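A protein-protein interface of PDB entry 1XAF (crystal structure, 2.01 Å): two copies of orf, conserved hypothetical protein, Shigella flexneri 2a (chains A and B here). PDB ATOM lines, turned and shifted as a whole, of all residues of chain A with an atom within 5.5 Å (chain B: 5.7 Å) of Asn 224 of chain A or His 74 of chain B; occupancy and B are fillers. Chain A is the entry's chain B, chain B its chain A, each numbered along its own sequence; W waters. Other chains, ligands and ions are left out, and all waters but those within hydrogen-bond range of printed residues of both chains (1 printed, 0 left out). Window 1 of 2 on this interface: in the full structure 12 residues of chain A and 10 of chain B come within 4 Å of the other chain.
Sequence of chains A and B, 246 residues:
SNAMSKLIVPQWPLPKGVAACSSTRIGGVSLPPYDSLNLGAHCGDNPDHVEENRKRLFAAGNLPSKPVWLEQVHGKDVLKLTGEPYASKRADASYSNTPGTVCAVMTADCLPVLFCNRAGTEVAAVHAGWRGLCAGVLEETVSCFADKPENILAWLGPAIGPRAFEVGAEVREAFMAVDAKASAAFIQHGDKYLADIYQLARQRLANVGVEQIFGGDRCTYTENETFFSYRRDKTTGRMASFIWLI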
ATOM      1  N   ARG A  25     -26.669  36.390 -19.521  1.00  0.00           N
ATOM      2  CA  ARG A  25     -27.340  37.338 -18.629  1.00  0.00           C
ATOM      3  C   ARG A  25     -26.458  38.481 -18.121  1.00  0.00           C
ATOM      4  O   ARG A  25     -26.946  39.401 -17.420  1.00  0.00           O
ATOM      5  CB  ARG A  25     -28.007  36.599 -17.486  1.00  0.00           C
ATOM      6  CG  ARG A  25     -27.076  36.148 -16.367  1.00  0.00           C
ATOM      7  CD  ARG A  25     -27.878  35.434 -15.331  1.00  0.00           C
ATOM      8  NE  ARG A  25     -28.932  36.271 -14.734  1.00  0.00           N
ATOM      9  CZ  ARG A  25     -29.879  35.778 -13.938  1.00  0.00           C
ATOM     10  NH1 ARG A  25     -29.879  34.485 -13.684  1.00  0.00           N
ATOM     11  NH2 ARG A  25     -30.817  36.556 -13.392  1.00  0.00           N
ATOM     12  N   THR A 220     -29.039  26.098 -19.628  1.00  0.00           N
ATOM     13  CA  THR A 220     -29.571  27.352 -19.103  1.00  0.00           C
ATOM     14  C   THR A 220     -30.067  27.242 -17.644  1.00  0.00           C
ATOM     15  O   THR A 220     -29.963  28.203 -16.896  1.00  0.00           O
ATOM     16  CB  THR A 220     -30.703  27.881 -19.973  1.00  0.00           C
ATOM     17  OG1 THR A 220     -31.703  26.886 -20.035  1.00  0.00           O
ATOM     18  CG2 THR A 220     -30.220  28.212 -21.400  1.00  0.00           C
ATOM     19  N   TYR A 221     -30.656  26.103 -17.279  1.00  0.00           N
ATOM     20  CA  TYR A 221     -31.161  25.827 -15.913  1.00  0.00           C
ATOM     21  C   TYR A 221     -30.035  25.716 -14.840  1.00  0.00           C
ATOM     22  O   TYR A 221     -30.127  26.326 -13.770  1.00  0.00           O
ATOM     23  CB  TYR A 221     -32.002  24.542 -15.917  1.00  0.00           C
ATOM     24  CG  TYR A 221     -32.832  24.333 -14.660  1.00  0.00           C
ATOM     25  CD1 TYR A 221     -34.175  24.711 -14.621  1.00  0.00           C
ATOM     26  CD2 TYR A 221     -32.274  23.761 -13.509  1.00  0.00           C
ATOM     27  CE1 TYR A 221     -34.928  24.536 -13.472  1.00  0.00           C
ATOM     28  CE2 TYR A 221     -33.030  23.598 -12.363  1.00  0.00           C
ATOM     29  CZ  TYR A 221     -34.345  24.005 -12.344  1.00  0.00           C
ATOM     30  OH  TYR A 221     -35.121  23.840 -11.202  1.00  0.00           O
ATOM     31  N   THR A 222     -28.991  24.942 -15.132  1.00  0.00           N
ATOM     32  CA  THR A 222     -27.819  24.767 -14.234  1.00  0.00           C
ATOM     33  C   THR A 222     -27.018  26.048 -14.021  1.00  0.00           C
ATOM     34  O   THR A 222     -26.720  26.407 -12.874  1.00  0.00           O
ATOM     35  CB  THR A 222     -26.800  23.711 -14.799  1.00  0.00           C
ATOM     36  OG1 THR A 222     -27.467  22.467 -15.016  1.00  0.00           O
ATOM     37  CG2 THR A 222     -25.624  23.462 -13.834  1.00  0.00           C
ATOM     38  N   GLU A 223     -26.652  26.703 -15.129  1.00  0.00           N
ATOM     39  CA  GLU A 223     -25.646  27.761 -15.137  1.00  0.00           C
ATOM     40  C   GLU A 223     -26.313  29.081 -14.831  1.00  0.00           C
ATOM     41  O   GLU A 223     -26.370  29.970 -15.666  1.00  0.00           O
ATOM     42  CB  GLU A 223     -24.901  27.784 -16.481  1.00  0.00           C
ATOM     43  CG  GLU A 223     -24.411  26.393 -16.931  1.00  0.00           C
ATOM     44  CD  GLU A 223     -23.455  26.432 -18.128  1.00  0.00           C
ATOM     45  OE1 GLU A 223     -22.325  26.958 -17.988  1.00  0.00           O
ATOM     46  OE2 GLU A 223     -23.824  25.914 -19.202  1.00  0.00           O
ATOM     47  N   ASN A 224     -26.828  29.201 -13.609  1.00  0.00           N
ATOM     48  CA  ASN A 224     -27.673  30.344 -13.255  1.00  0.00           C
ATOM     49  C   ASN A 224     -26.957  31.690 -13.229  1.00  0.00           C
ATOM     50  O   ASN A 224     -27.586  32.735 -13.332  1.00  0.00           O
ATOM     51  CB  ASN A 224     -28.495  30.069 -11.992  1.00  0.00           C
ATOM     52  CG  ASN A 224     -27.667  29.581 -10.848  1.00  0.00           C
ATOM     53  OD1 ASN A 224     -26.876  30.329 -10.285  1.00  0.00           O
ATOM     54  ND2 ASN A 224     -27.855  28.327 -10.475  1.00  0.00           N
ATOM     55  N   GLU A 225     -25.632  31.653 -13.119  1.00  0.00           N
ATOM     56  CA  GLU A 225     -24.831  32.887 -13.178  1.00  0.00           C
ATOM     57  C   GLU A 225     -24.634  33.398 -14.595  1.00  0.00           C
ATOM     58  O   GLU A 225     -24.330  34.564 -14.777  1.00  0.00           O
ATOM     59  CB  GLU A 225     -23.450  32.687 -12.520  1.00  0.00           C
ATOM     60  CG  GLU A 225     -23.495  32.115 -11.103  1.00  0.00           C
ATOM     61  CD  GLU A 225     -23.902  33.125 -10.029  1.00  0.00           C
ATOM     62  OE1 GLU A 225     -24.466  34.204 -10.348  1.00  0.00           O
ATOM     63  OE2 GLU A 225     -23.656  32.818  -8.838  1.00  0.00           O
ATOM     64  N   THR A 226     -24.817  32.526 -15.590  1.00  0.00           N
ATOM     65  CA  THR A 226     -24.647  32.875 -17.012  1.00  0.00           C
ATOM     66  C   THR A 226     -25.959  33.043 -17.788  1.00  0.00           C
ATOM     67  O   THR A 226     -26.031  33.858 -18.713  1.00  0.00           O
ATOM     68  CB  THR A 226     -23.749  31.796 -17.698  1.00  0.00           C
ATOM     69  OG1 THR A 226     -22.506  31.749 -17.018  1.00  0.00           O
ATOM     70  CG2 THR A 226     -23.461  32.108 -19.144  1.00  0.00           C
ATOM     71  N   PHE A 227     -26.989  32.284 -17.434  1.00  0.00           N
ATOM     72  CA  PHE A 227     -28.228  32.267 -18.215  1.00  0.00           C
ATOM     73  C   PHE A 227     -29.492  32.499 -17.423  1.00  0.00           C
ATOM     74  O   PHE A 227     -29.616  32.007 -16.307  1.00  0.00           O
ATOM     75  CB  PHE A 227     -28.394  30.917 -18.937  1.00  0.00           C
ATOM     76  CG  PHE A 227     -27.259  30.564 -19.832  1.00  0.00           C
ATOM     77  CD1 PHE A 227     -27.013  31.313 -21.020  1.00  0.00           C
ATOM     78  CD2 PHE A 227     -26.455  29.452 -19.540  1.00  0.00           C
ATOM     79  CE1 PHE A 227     -25.952  30.993 -21.854  1.00  0.00           C
ATOM     80  CE2 PHE A 227     -25.377  29.115 -20.386  1.00  0.00           C
ATOM     81  CZ  PHE A 227     -25.128  29.867 -21.546  1.00  0.00           C
ATOM     82  N   ARG A 232     -36.555  27.612 -14.327  1.00  0.00           N
ATOM     83  CA  ARG A 232     -36.001  27.911 -13.017  1.00  0.00           C
ATOM     84  C   ARG A 232     -36.677  29.145 -12.367  1.00  0.00           C
ATOM     85  O   ARG A 232     -37.140  29.078 -11.211  1.00  0.00           O
ATOM     86  CB  ARG A 232     -34.479  28.092 -13.139  1.00  0.00           C
ATOM     87  CG  ARG A 232     -33.703  28.152 -11.808  1.00  0.00           C
ATOM     88  CD  ARG A 232     -32.237  28.556 -12.035  1.00  0.00           C
ATOM     89  NE  ARG A 232     -32.127  29.868 -12.675  1.00  0.00           N
ATOM     90  CZ  ARG A 232     -31.411  30.165 -13.768  1.00  0.00           C
ATOM     91  NH1 ARG A 232     -30.625  29.262 -14.370  1.00  0.00           N
ATOM     92  NH2 ARG A 232     -31.463  31.412 -14.240  1.00  0.00           N
ATOM     93  N   GLN B  72     -35.035  23.205  -5.829  1.00  0.00           N
ATOM     94  CA  GLN B  72     -34.359  24.466  -5.469  1.00  0.00           C
ATOM     95  C   GLN B  72     -34.037  25.279  -6.717  1.00  0.00           C
ATOM     96  O   GLN B  72     -33.412  24.766  -7.643  1.00  0.00           O
ATOM     97  CB  GLN B  72     -33.055  24.190  -4.706  1.00  0.00           C
ATOM     98  CG  GLN B  72     -33.288  23.462  -3.374  1.00  0.00           C
ATOM     99  CD  GLN B  72     -32.011  22.913  -2.745  1.00  0.00           C
ATOM    100  OE1 GLN B  72     -30.882  23.162  -3.213  1.00  0.00           O
ATOM    101  NE2 GLN B  72     -32.183  22.158  -1.701  1.00  0.00           N
ATOM    102  N   VAL B  73     -34.418  26.548  -6.706  1.00  0.00           N
ATOM    103  CA  VAL B  73     -34.286  27.399  -7.902  1.00  0.00           C
ATOM    104  C   VAL B  73     -33.404  28.643  -7.629  1.00  0.00           C
ATOM    105  O   VAL B  73     -33.345  29.580  -8.442  1.00  0.00           O
ATOM    106  CB  VAL B  73     -35.698  27.766  -8.469  1.00  0.00           C
ATOM    107  CG1 VAL B  73     -36.396  26.564  -9.058  1.00  0.00           C
ATOM    108  CG2 VAL B  73     -36.577  28.373  -7.417  1.00  0.00           C
ATOM    109  N   HIS B  74     -32.713  28.643  -6.485  1.00  0.00           N
ATOM    110  CA  HIS B  74     -31.872  29.773  -6.068  1.00  0.00           C
ATOM    111  C   HIS B  74     -32.649  31.057  -5.840  1.00  0.00           C
ATOM    112  O   HIS B  74     -32.105  32.154  -5.978  1.00  0.00           O
ATOM    113  CB  HIS B  74     -30.698  29.993  -7.035  1.00  0.00           C
ATOM    114  CG  HIS B  74     -29.621  28.968  -6.890  1.00  0.00           C
ATOM    115  ND1 HIS B  74     -29.723  27.712  -7.438  1.00  0.00           N
ATOM    116  CD2 HIS B  74     -28.458  28.985  -6.196  1.00  0.00           C
ATOM    117  CE1 HIS B  74     -28.648  27.005  -7.130  1.00  0.00           C
ATOM    118  NE2 HIS B  74     -27.856  27.761  -6.392  1.00  0.00           N
ATOM    119  N   GLY B  75     -33.922  30.919  -5.496  1.00  0.00           N
ATOM    120  CA  GLY B  75     -34.708  32.065  -5.080  1.00  0.00           C
ATOM    121  C   GLY B  75     -34.804  32.188  -3.578  1.00  0.00           C
ATOM    122  O   GLY B  75     -33.897  31.775  -2.852  1.00  0.00           O
ATOM    123  N   LYS B  76     -35.922  32.739  -3.112  1.00  0.00           N
ATOM    124  CA  LYS B  76     -36.112  33.053  -1.691  1.00  0.00           C
ATOM    125  C   LYS B  76     -37.413  32.501  -1.086  1.00  0.00           C
ATOM    126  O   LYS B  76     -37.807  32.908   0.025  1.00  0.00           O
ATOM    127  CB  LYS B  76     -36.104  34.572  -1.500  1.00  0.00           C
ATOM    128  CG  LYS B  76     -37.112  35.291  -2.478  1.00  0.00           C
ATOM    129  CD  LYS B  76     -37.301  36.756  -2.175  1.00  0.00           C
ATOM    130  CE  LYS B  76     -37.590  36.979  -0.688  1.00  0.00           C
ATOM    131  NZ  LYS B  76     -38.842  36.328  -0.253  1.00  0.00           N
ATOM    132  N   ASP B  92     -36.559  27.411  -1.873  1.00  0.00           N
ATOM    133  CA  ASP B  92     -35.167  27.258  -1.452  1.00  0.00           C
ATOM    134  C   ASP B  92     -35.023  27.148   0.060  1.00  0.00           C
ATOM    135  O   ASP B  92     -33.914  27.105   0.563  1.00  0.00           O
ATOM    136  CB  ASP B  92     -34.287  28.344  -2.050  1.00  0.00           C
ATOM    137  CG  ASP B  92     -34.014  28.115  -3.561  1.00  0.00           C
ATOM    138  OD1 ASP B  92     -32.959  27.514  -3.908  1.00  0.00           O
ATOM    139  OD2 ASP B  92     -34.867  28.532  -4.399  1.00  0.00           O
ATOM    140  N   CYS B 110     -23.228  26.739  -1.912  1.00  0.00           N
ATOM    141  CA  CYS B 110     -24.206  27.639  -1.291  1.00  0.00           C
ATOM    142  C   CYS B 110     -24.319  27.396   0.204  1.00  0.00           C
ATOM    143  O   CYS B 110     -24.038  26.319   0.709  1.00  0.00           O
ATOM    144  CB  CYS B 110     -25.574  27.597  -1.963  1.00  0.00           C
ATOM    145  SG  CYS B 110     -25.513  28.058  -3.738  1.00  0.00           S
ATOM    146  N   HIS B 127     -31.459  26.812   1.733  1.00  0.00           N
ATOM    147  CA  HIS B 127     -30.410  26.817   0.729  1.00  0.00           C
ATOM    148  C   HIS B 127     -30.190  28.286   0.304  1.00  0.00           C
ATOM    149  O   HIS B 127     -30.958  28.867  -0.448  1.00  0.00           O
ATOM    150  CB  HIS B 127     -30.739  25.873  -0.444  1.00  0.00           C
ATOM    151  CG  HIS B 127     -30.022  26.187  -1.734  1.00  0.00           C
ATOM    152  ND1 HIS B 127     -30.677  26.697  -2.838  1.00  0.00           N
ATOM    153  CD2 HIS B 127     -28.722  26.067  -2.098  1.00  0.00           C
ATOM    154  CE1 HIS B 127     -29.816  26.868  -3.826  1.00  0.00           C
ATOM    155  NE2 HIS B 127     -28.620  26.501  -3.401  1.00  0.00           N
ATOM    156  N   GLY B 129     -28.168  30.547  -1.643  1.00  0.00           N
ATOM    157  CA  GLY B 129     -27.294  31.105  -2.678  1.00  0.00           C
ATOM    158  C   GLY B 129     -27.192  32.603  -2.466  1.00  0.00           C
ATOM    159  O   GLY B 129     -28.015  33.183  -1.751  1.00  0.00           O
ATOM    160  N   ARG B 131     -27.952  35.073  -4.416  1.00  0.00           N
ATOM    161  CA  ARG B 131     -29.125  35.797  -4.914  1.00  0.00           C
ATOM    162  C   ARG B 131     -30.271  35.729  -3.892  1.00  0.00           C
ATOM    163  O   ARG B 131     -30.919  36.726  -3.608  1.00  0.00           O
ATOM    164  CB  ARG B 131     -29.573  35.283  -6.290  1.00  0.00           C
ATOM    165  CG  ARG B 131     -28.790  35.845  -7.472  1.00  0.00           C
ATOM    166  CD  ARG B 131     -29.503  35.645  -8.854  1.00  0.00           C
ATOM    167  NE  ARG B 131     -28.961  36.587  -9.845  1.00  0.00           N
ATOM    168  CZ  ARG B 131     -27.988  36.291 -10.700  1.00  0.00           C
ATOM    169  NH1 ARG B 131     -27.486  35.061 -10.759  1.00  0.00           N
ATOM    170  NH2 ARG B 131     -27.515  37.215 -11.520  1.00  0.00           N
ATOM    171  N   GLY B 132     -30.491  34.545  -3.330  1.00  0.00           N
ATOM    172  CA  GLY B 132     -31.557  34.327  -2.374  1.00  0.00           C
ATOM    173  C   GLY B 132     -31.250  34.982  -1.042  1.00  0.00           C
ATOM    174  O   GLY B 132     -32.127  35.564  -0.419  1.00  0.00           O
HETATM  175  O   HOH W   1     -27.882  32.753  -8.971  1.00  0.00           O
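The guanidinium group of Arg 131 of chain B is in hydrogen-bond range of the backbone carbonyl oxygen of Asn 224 of chain A.
The side-chain carboxylate (OE1) of Glu 225 of chain A lies within salt-bridge range of the guanidinium group (NH1) of Arg 131 of chain B (3.2 Å).
The backbone NH (N) of Val 73 of chain B sits at hydrogen-bond distance from the side-chain carboxylate (OD2) of Asp 92 of chain B, at 3.1 Å.
The guanidinium group (NH1) of Arg 25 of chain A lies within hydrogen-bond range of the backbone carbonyl oxygen (O) of Asn 224 of chain A (2.9 Å).
NH1 of Arg 232 of chain A lies within hydrogen-bond range of O of Thr 220 of chain A (2.8 Å).
O of Tyr 221 of chain A sits at hydrogen-bond distance from NH1 of Arg 232 of chain A (3.0 Å).
The backbone carbonyl oxygen (O) of Thr 222 of chain A is in hydrogen-bond range of the side-chain amide nitrogen (ND2) of Asn 224 of chain A, at 3.3 Å.
O of Phe 227 of chain A lies within hydrogen-bond range of NH2 of Arg 232 of chain A (2.8 Å).
Arg 25 of chain A touches Arg 131 of chain B.
Tyr 221 of chain A touches Val 73 of chain B (OH to CG1, 3.7 Å).
His 74 of chain B touches Asn 224 of chain A (ND1 to ND2, 3.6 Å).
Arg 232 of chain A touches Val 73 of chain B.
Of the printed residues of chain B, Arg 25 of chain A touches Arg 131 (3.6 Å).
Of the printed residues of chain B, Glu 225 of chain A touches Arg 131 (3.2 Å).
Of the printed residues of chain B, Arg 232 of chain A touches Val 73.
Printed residues of chain A within 4 Å of Val 73 of chain B: Tyr 221 and Arg 232.
Of chain A, only Asn 224 comes within 4 Å of His 74 of chain B.
Of the printed residues of chain A, Arg 131 of chain B touches Arg 25 (3.6 Å), Asn 224 (3.5 Å) and Glu 225 (3.2 Å).
The nearest printed residue of chain B that does not touch Asn 224 of chain A is Val 73 of chain B (6.0 Å).
The nearest printed residue of chain A that does not touch Val 73 of chain B is Asn 224 of chain A (6.0 Å).
Hydrophobic or aromatic side chains of chain B within 4 Å of the printed part of chain A: Val 73 and His 74.
Hydrophobic or aromatic side chains of chain A that line the printed part of chain B: Tyr 221.
Among the printed residues, Asp or Glu carboxylates within 4 Å of a Lys or Arg side-chain nitrogen of the other chain: Glu 225 of chain A with Arg 131 of chain B.
No position is printed for both chains.
Of the 6 pairs that touch across the chains among the printed residues, none has its exchanged pair printed and touching as well.
Water W1 bridges the side-chain amide oxygen of Asn 224 of chain A (2.9 Å) and the guanidinium group of Arg 131 of chain B (2.9 Å).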
